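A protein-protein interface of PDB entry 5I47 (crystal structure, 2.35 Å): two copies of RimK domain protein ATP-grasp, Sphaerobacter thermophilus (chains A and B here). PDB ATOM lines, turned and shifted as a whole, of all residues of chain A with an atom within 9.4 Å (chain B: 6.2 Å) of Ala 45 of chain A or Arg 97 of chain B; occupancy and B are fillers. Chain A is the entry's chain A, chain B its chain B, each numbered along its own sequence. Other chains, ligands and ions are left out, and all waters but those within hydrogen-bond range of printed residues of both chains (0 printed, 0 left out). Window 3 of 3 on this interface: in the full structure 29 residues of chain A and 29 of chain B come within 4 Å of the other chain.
No position is printed for both chains.
O of Pro 44 of chain A sits at hydrogen-bond distance from NH2 of Arg 97 of chain B (3.3 Å).
Pro 44 of chain A touches Leu 96 of chain B (CG to CD2, 3.6 Å). CB of Pro 44 of chain A touches CD1 of Ile 100 of chain B, at 3.8 Å. Ala 45 of chain A touches Arg 97 of chain B. Met 93 of chain B touches Val 67 of chain A (CG to CG1, 3.7 Å).
Printed residues of chain A that touch a printed residue of chain B: Pro 44, Ala 45 and Val 67. Along chain A the printed residues that touch a printed residue of chain B span positions 44 to 67. Of the 11 printed residues of chain B, 4 touch a printed residue of chain A. Printed residues of chain B that touch a printed residue of chain A: Met 93, Leu 96, Arg 97 and Ile 100. Hydrophobic or aromatic side chains of chain B that line the printed part of chain A: Met 93, Leu 96 and Ile 100.
Ser 43 of chain A touches none of the printed residues of chain B. Printed residues of chain B within 4 Å of Pro 44 of chain A: Leu 96, Arg 97 and Ile 100. Of the printed residues of chain B, Ala 45 of chain A touches Arg 97. Of the printed residues of chain B, Val 67 of chain A touches Met 93 (3.7 Å). Ala 73 of chain A touches none of the printed residues of chain B. Of the printed residues of chain A, Met 93 of chain B touches Val 67. Leu 96 of chain B touches just one residue of chain A: Pro 44. Of chain A, only Pro 44 comes within 4 Å of Ile 100 of chain B. The nearest printed residue of chain A that does not touch Arg 97 of chain B is Ser 74 of chain A (4.4 Å). The nearest printed residue of chain B that does not touch Val 67 of chain A is Ala 94 of chain B (6.8 Å).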
ATOM      1  N   LEU A  42      -7.675   5.960   7.074  1.00  0.00           N
ATOM      2  CA  LEU A  42      -6.410   6.465   6.560  1.00  0.00           C
ATOM      3  C   LEU A  42      -6.127   5.909   5.171  1.00  0.00           C
ATOM      4  O   LEU A  42      -6.339   4.724   4.907  1.00  0.00           O
ATOM      5  CB  LEU A  42      -5.262   6.104   7.504  1.00  0.00           C
ATOM      6  CG  LEU A  42      -5.483   6.495   8.965  1.00  0.00           C
ATOM      7  CD1 LEU A  42      -4.367   5.965   9.848  1.00  0.00           C
ATOM      8  CD2 LEU A  42      -5.594   7.991   9.094  1.00  0.00           C
ATOM      9  N   SER A  43      -5.640   6.773   4.294  1.00  0.00           N
ATOM     10  CA  SER A  43      -5.174   6.333   2.986  1.00  0.00           C
ATOM     11  C   SER A  43      -3.763   5.772   3.113  1.00  0.00           C
ATOM     12  O   SER A  43      -2.882   6.451   3.649  1.00  0.00           O
ATOM     13  CB  SER A  43      -5.190   7.491   1.992  1.00  0.00           C
ATOM     14  OG  SER A  43      -4.634   7.103   0.745  1.00  0.00           O
ATOM     15  N   PRO A  44      -3.514   4.547   2.645  1.00  0.00           N
ATOM     16  CA  PRO A  44      -2.171   3.965   2.797  1.00  0.00           C
ATOM     17  C   PRO A  44      -1.096   4.720   2.040  1.00  0.00           C
ATOM     18  O   PRO A  44       0.074   4.676   2.438  1.00  0.00           O
ATOM     19  CB  PRO A  44      -2.343   2.541   2.249  1.00  0.00           C
ATOM     20  CG  PRO A  44      -3.806   2.286   2.284  1.00  0.00           C
ATOM     21  CD  PRO A  44      -4.454   3.603   2.025  1.00  0.00           C
ATOM     22  N   ALA A  45      -1.453   5.401   0.949  1.00  0.00           N
ATOM     23  CA  ALA A  45      -0.461   6.146   0.181  1.00  0.00           C
ATOM     24  C   ALA A  45       0.196   7.222   1.038  1.00  0.00           C
ATOM     25  O   ALA A  45       1.426   7.273   1.156  1.00  0.00           O
ATOM     26  CB  ALA A  45      -1.114   6.757  -1.061  1.00  0.00           C
ATOM     27  N   ALA A  46      -0.612   8.084   1.656  1.00  0.00           N
ATOM     28  CA  ALA A  46      -0.117   9.117   2.565  1.00  0.00           C
ATOM     29  C   ALA A  46      -1.114   9.286   3.704  1.00  0.00           C
ATOM     30  O   ALA A  46      -2.038  10.106   3.623  1.00  0.00           O
ATOM     31  CB  ALA A  46       0.115  10.439   1.835  1.00  0.00           C
ATOM     32  N   PRO A  47      -0.963   8.520   4.781  1.00  0.00           N
ATOM     33  CA  PRO A  47      -1.931   8.589   5.882  1.00  0.00           C
ATOM     34  C   PRO A  47      -1.755   9.824   6.753  1.00  0.00           C
ATOM     35  O   PRO A  47      -0.650  10.341   6.939  1.00  0.00           O
ATOM     36  CB  PRO A  47      -1.654   7.310   6.682  1.00  0.00           C
ATOM     37  CG  PRO A  47      -0.262   6.945   6.349  1.00  0.00           C
ATOM     38  CD  PRO A  47       0.004   7.422   4.956  1.00  0.00           C
ATOM     39  N   SER A  48      -2.878  10.287   7.298  1.00  0.00           N
ATOM     40  CA  SER A  48      -2.903  11.490   8.115  1.00  0.00           C
ATOM     41  C   SER A  48      -4.172  11.496   8.948  1.00  0.00           C
ATOM     42  O   SER A  48      -5.249  11.176   8.445  1.00  0.00           O
ATOM     43  CB  SER A  48      -2.837  12.753   7.252  1.00  0.00           C
ATOM     44  OG  SER A  48      -3.033  13.915   8.038  1.00  0.00           O
ATOM     45  N   VAL A  67       0.139  -1.100  13.963  1.00  0.00           N
ATOM     46  CA  VAL A  67      -0.114  -0.689  12.584  1.00  0.00           C
ATOM     47  C   VAL A  67      -0.430   0.801  12.518  1.00  0.00           C
ATOM     48  O   VAL A  67       0.096   1.527  11.665  1.00  0.00           O
ATOM     49  CB  VAL A  67      -1.253  -1.534  11.985  1.00  0.00           C
ATOM     50  CG1 VAL A  67      -1.682  -0.977  10.641  1.00  0.00           C
ATOM     51  CG2 VAL A  67      -0.817  -2.985  11.853  1.00  0.00           C
ATOM     52  N   ALA A  70       2.732   2.811  12.873  1.00  0.00           N
ATOM     53  CA  ALA A  70       3.522   2.785  11.646  1.00  0.00           C
ATOM     54  C   ALA A  70       2.860   3.596  10.542  1.00  0.00           C
ATOM     55  O   ALA A  70       3.546   4.276   9.770  1.00  0.00           O
ATOM     56  CB  ALA A  70       3.738   1.342  11.191  1.00  0.00           C
ATOM     57  N   LEU A  71       1.531   3.540  10.452  1.00  0.00           N
ATOM     58  CA  LEU A  71       0.820   4.295   9.424  1.00  0.00           C
ATOM     59  C   LEU A  71       1.037   5.790   9.596  1.00  0.00           C
ATOM     60  O   LEU A  71       1.588   6.455   8.713  1.00  0.00           O
ATOM     61  CB  LEU A  71      -0.674   3.970   9.466  1.00  0.00           C
ATOM     62  CG  LEU A  71      -1.176   2.907   8.497  1.00  0.00           C
ATOM     63  CD1 LEU A  71      -2.685   2.771   8.596  1.00  0.00           C
ATOM     64  CD2 LEU A  71      -0.744   3.257   7.078  1.00  0.00           C
ATOM     65  N   LEU A  72       0.611   6.334  10.740  1.00  0.00           N
ATOM     66  CA  LEU A  72       0.682   7.777  10.948  1.00  0.00           C
ATOM     67  C   LEU A  72       2.115   8.293  10.858  1.00  0.00           C
ATOM     68  O   LEU A  72       2.342   9.402  10.362  1.00  0.00           O
ATOM     69  CB  LEU A  72       0.059   8.139  12.298  1.00  0.00           C
ATOM     70  CG  LEU A  72      -1.454   7.934  12.426  1.00  0.00           C
ATOM     71  CD1 LEU A  72      -1.928   8.237  13.840  1.00  0.00           C
ATOM     72  CD2 LEU A  72      -2.195   8.801  11.424  1.00  0.00           C
ATOM     73  N   ALA A  73       3.092   7.508  11.319  1.00  0.00           N
ATOM     74  CA  ALA A  73       4.482   7.923  11.172  1.00  0.00           C
ATOM     75  C   ALA A  73       4.898   7.978   9.707  1.00  0.00           C
ATOM     76  O   ALA A  73       5.691   8.848   9.327  1.00  0.00           O
ATOM     77  CB  ALA A  73       5.403   6.985  11.951  1.00  0.00           C
ATOM     78  N   SER A  74       4.369   7.070   8.873  1.00  0.00           N
ATOM     79  CA  SER A  74       4.714   7.067   7.451  1.00  0.00           C
ATOM     80  C   SER A  74       4.309   8.361   6.761  1.00  0.00           C
ATOM     81  O   SER A  74       4.974   8.789   5.813  1.00  0.00           O
ATOM     82  CB  SER A  74       4.051   5.886   6.742  1.00  0.00           C
ATOM     83  OG  SER A  74       4.767   4.690   6.974  1.00  0.00           O
ATOM     84  N   GLY A  75       3.220   8.982   7.202  1.00  0.00           N
ATOM     85  CA  GLY A  75       2.737  10.212   6.619  1.00  0.00           C
ATOM     86  C   GLY A  75       3.301  11.469   7.223  1.00  0.00           C
ATOM     87  O   GLY A  75       2.898  12.567   6.831  1.00  0.00           O
ATOM     88  N   GLY A  76       4.219  11.352   8.176  1.00  0.00           N
ATOM     89  CA  GLY A  76       4.864  12.506   8.762  1.00  0.00           C
ATOM     90  C   GLY A  76       4.384  12.902  10.138  1.00  0.00           C
ATOM     91  O   GLY A  76       4.790  13.958  10.630  1.00  0.00           O
ATOM     92  N   ARG B  92      -2.311  -8.435   5.332  1.00  0.00           N
ATOM     93  CA  ARG B  92      -2.769  -7.655   4.188  1.00  0.00           C
ATOM     94  C   ARG B  92      -2.247  -6.227   4.237  1.00  0.00           C
ATOM     95  O   ARG B  92      -2.013  -5.616   3.188  1.00  0.00           O
ATOM     96  CB  ARG B  92      -4.298  -7.664   4.120  1.00  0.00           C
ATOM     97  CG  ARG B  92      -4.894  -9.055   3.905  1.00  0.00           C
ATOM     98  CD  ARG B  92      -6.344  -9.003   3.424  1.00  0.00           C
ATOM     99  NE  ARG B  92      -6.880 -10.347   3.230  1.00  0.00           N
ATOM    100  CZ  ARG B  92      -7.684 -10.962   4.090  1.00  0.00           C
ATOM    101  NH1 ARG B  92      -8.070 -10.348   5.197  1.00  0.00           N
ATOM    102  NH2 ARG B  92      -8.109 -12.192   3.836  1.00  0.00           N
ATOM    103  N   MET B  93      -2.051  -5.681   5.432  1.00  0.00           N
ATOM    104  CA  MET B  93      -1.567  -4.315   5.576  1.00  0.00           C
ATOM    105  C   MET B  93      -0.112  -4.193   5.136  1.00  0.00           C
ATOM    106  O   MET B  93       0.250  -3.271   4.400  1.00  0.00           O
ATOM    107  CB  MET B  93      -1.716  -3.846   7.023  1.00  0.00           C
ATOM    108  CG  MET B  93      -1.196  -2.444   7.268  1.00  0.00           C
ATOM    109  SD  MET B  93      -2.276  -1.085   6.370  1.00  0.00           S
ATOM    110  CE  MET B  93      -0.987  -0.424   5.052  1.00  0.00           C
ATOM    111  N   ALA B  94       0.728  -5.126   5.593  1.00  0.00           N
ATOM    112  CA  ALA B  94       2.137  -5.085   5.211  1.00  0.00           C
ATOM    113  C   ALA B  94       2.307  -5.359   3.722  1.00  0.00           C
ATOM    114  O   ALA B  94       3.134  -4.722   3.059  1.00  0.00           O
ATOM    115  CB  ALA B  94       2.944  -6.084   6.042  1.00  0.00           C
ATOM    116  N   LEU B  95       1.527  -6.300   3.181  1.00  0.00           N
ATOM    117  CA  LEU B  95       1.560  -6.560   1.744  1.00  0.00           C
ATOM    118  C   LEU B  95       1.107  -5.338   0.959  1.00  0.00           C
ATOM    119  O   LEU B  95       1.710  -4.987  -0.063  1.00  0.00           O
ATOM    120  CB  LEU B  95       0.679  -7.759   1.409  1.00  0.00           C
ATOM    121  CG  LEU B  95       0.545  -8.111  -0.075  1.00  0.00           C
ATOM    122  CD1 LEU B  95       1.894  -8.492  -0.670  1.00  0.00           C
ATOM    123  CD2 LEU B  95      -0.464  -9.234  -0.266  1.00  0.00           C
ATOM    124  N   LEU B  96       0.053  -4.669   1.432  1.00  0.00           N
ATOM    125  CA  LEU B  96      -0.454  -3.486   0.747  1.00  0.00           C
ATOM    126  C   LEU B  96       0.599  -2.385   0.690  1.00  0.00           C
ATOM    127  O   LEU B  96       0.830  -1.785  -0.365  1.00  0.00           O
ATOM    128  CB  LEU B  96      -1.721  -2.988   1.440  1.00  0.00           C
ATOM    129  CG  LEU B  96      -2.297  -1.669   0.924  1.00  0.00           C
ATOM    130  CD1 LEU B  96      -2.631  -1.780  -0.564  1.00  0.00           C
ATOM    131  CD2 LEU B  96      -3.527  -1.269   1.738  1.00  0.00           C
ATOM    132  N   ARG B  97       1.251  -2.097   1.818  1.00  0.00           N
ATOM    133  CA  ARG B  97       2.269  -1.054   1.801  1.00  0.00           C
ATOM    134  C   ARG B  97       3.469  -1.461   0.954  1.00  0.00           C
ATOM    135  O   ARG B  97       4.087  -0.606   0.309  1.00  0.00           O
ATOM    136  CB  ARG B  97       2.699  -0.710   3.230  1.00  0.00           C
ATOM    137  CG  ARG B  97       3.705   0.449   3.343  1.00  0.00           C
ATOM    138  CD  ARG B  97       3.212   1.744   2.680  1.00  0.00           C
ATOM    139  NE  ARG B  97       4.127   2.861   2.921  1.00  0.00           N
ATOM    140  CZ  ARG B  97       4.088   4.020   2.269  1.00  0.00           C
ATOM    141  NH1 ARG B  97       4.964   4.979   2.554  1.00  0.00           N
ATOM    142  NH2 ARG B  97       3.182   4.221   1.323  1.00  0.00           N
ATOM    143  N   HIS B  98       3.794  -2.757   0.919  1.00  0.00           N
ATOM    144  CA  HIS B  98       4.925  -3.216   0.119  1.00  0.00           C
ATOM    145  C   HIS B  98       4.652  -3.073  -1.372  1.00  0.00           C
ATOM    146  O   HIS B  98       5.529  -2.640  -2.129  1.00  0.00           O
ATOM    147  CB  HIS B  98       5.245  -4.670   0.467  1.00  0.00           C
ATOM    148  CG  HIS B  98       6.625  -5.096   0.075  1.00  0.00           C
ATOM    149  ND1 HIS B  98       6.941  -5.520  -1.198  1.00  0.00           N
ATOM    150  CD2 HIS B  98       7.774  -5.162   0.791  1.00  0.00           C
ATOM    151  CE1 HIS B  98       8.224  -5.829  -1.251  1.00  0.00           C
ATOM    152  NE2 HIS B  98       8.753  -5.621  -0.057  1.00  0.00           N
ATOM    153  N   LEU B  99       3.443  -3.436  -1.814  1.00  0.00           N
ATOM    154  CA  LEU B  99       3.100  -3.306  -3.229  1.00  0.00           C
ATOM    155  C   LEU B  99       3.032  -1.843  -3.651  1.00  0.00           C
ATOM    156  O   LEU B  99       3.449  -1.490  -4.760  1.00  0.00           O
ATOM    157  CB  LEU B  99       1.772  -4.013  -3.509  1.00  0.00           C
ATOM    158  CG  LEU B  99       1.780  -5.528  -3.288  1.00  0.00           C
ATOM    159  CD1 LEU B  99       0.377  -6.087  -3.376  1.00  0.00           C
ATOM    160  CD2 LEU B  99       2.702  -6.231  -4.287  1.00  0.00           C
ATOM    161  N   ILE B 100       2.515  -0.975  -2.778  1.00  0.00           N
ATOM    162  CA  ILE B 100       2.468   0.453  -3.083  1.00  0.00           C
ATOM    163  C   ILE B 100       3.876   1.006  -3.266  1.00  0.00           C
ATOM    164  O   ILE B 100       4.165   1.704  -4.246  1.00  0.00           O
ATOM    165  CB  ILE B 100       1.701   1.210  -1.984  1.00  0.00           C
ATOM    166  CG1 ILE B 100       0.213   0.840  -2.020  1.00  0.00           C
ATOM    167  CG2 ILE B 100       1.903   2.714  -2.124  1.00  0.00           C
ATOM    168  CD1 ILE B 100      -0.624   1.585  -1.011  1.00  0.00           C
ATOM    169  N   LEU B 101       4.776   0.710  -2.323  1.00  0.00           N
ATOM    170  CA  LEU B 101       6.153   1.179  -2.441  1.00  0.00           C
ATOM    171  C   LEU B 101       6.859   0.595  -3.659  1.00  0.00           C
ATOM    172  O   LEU B 101       7.806   1.205  -4.161  1.00  0.00           O
ATOM    173  CB  LEU B 101       6.939   0.846  -1.171  1.00  0.00           C
ATOM    174  CG  LEU B 101       6.616   1.708   0.047  1.00  0.00           C
ATOM    175  CD1 LEU B 101       7.226   1.114   1.293  1.00  0.00           C
ATOM    176  CD2 LEU B 101       7.112   3.129  -0.159  1.00  0.00           C
ATOM    177  N   ALA B 102       6.422  -0.566  -4.143  1.00  0.00           N
ATOM    178  CA  ALA B 102       6.974  -1.185  -5.342  1.00  0.00           C
ATOM    179  C   ALA B 102       6.313  -0.699  -6.623  1.00  0.00           C
ATOM    180  O   ALA B 102       6.649  -1.201  -7.699  1.00  0.00           O
ATOM    181  CB  ALA B 102       6.850  -2.709  -5.255  1.00  0.00           C
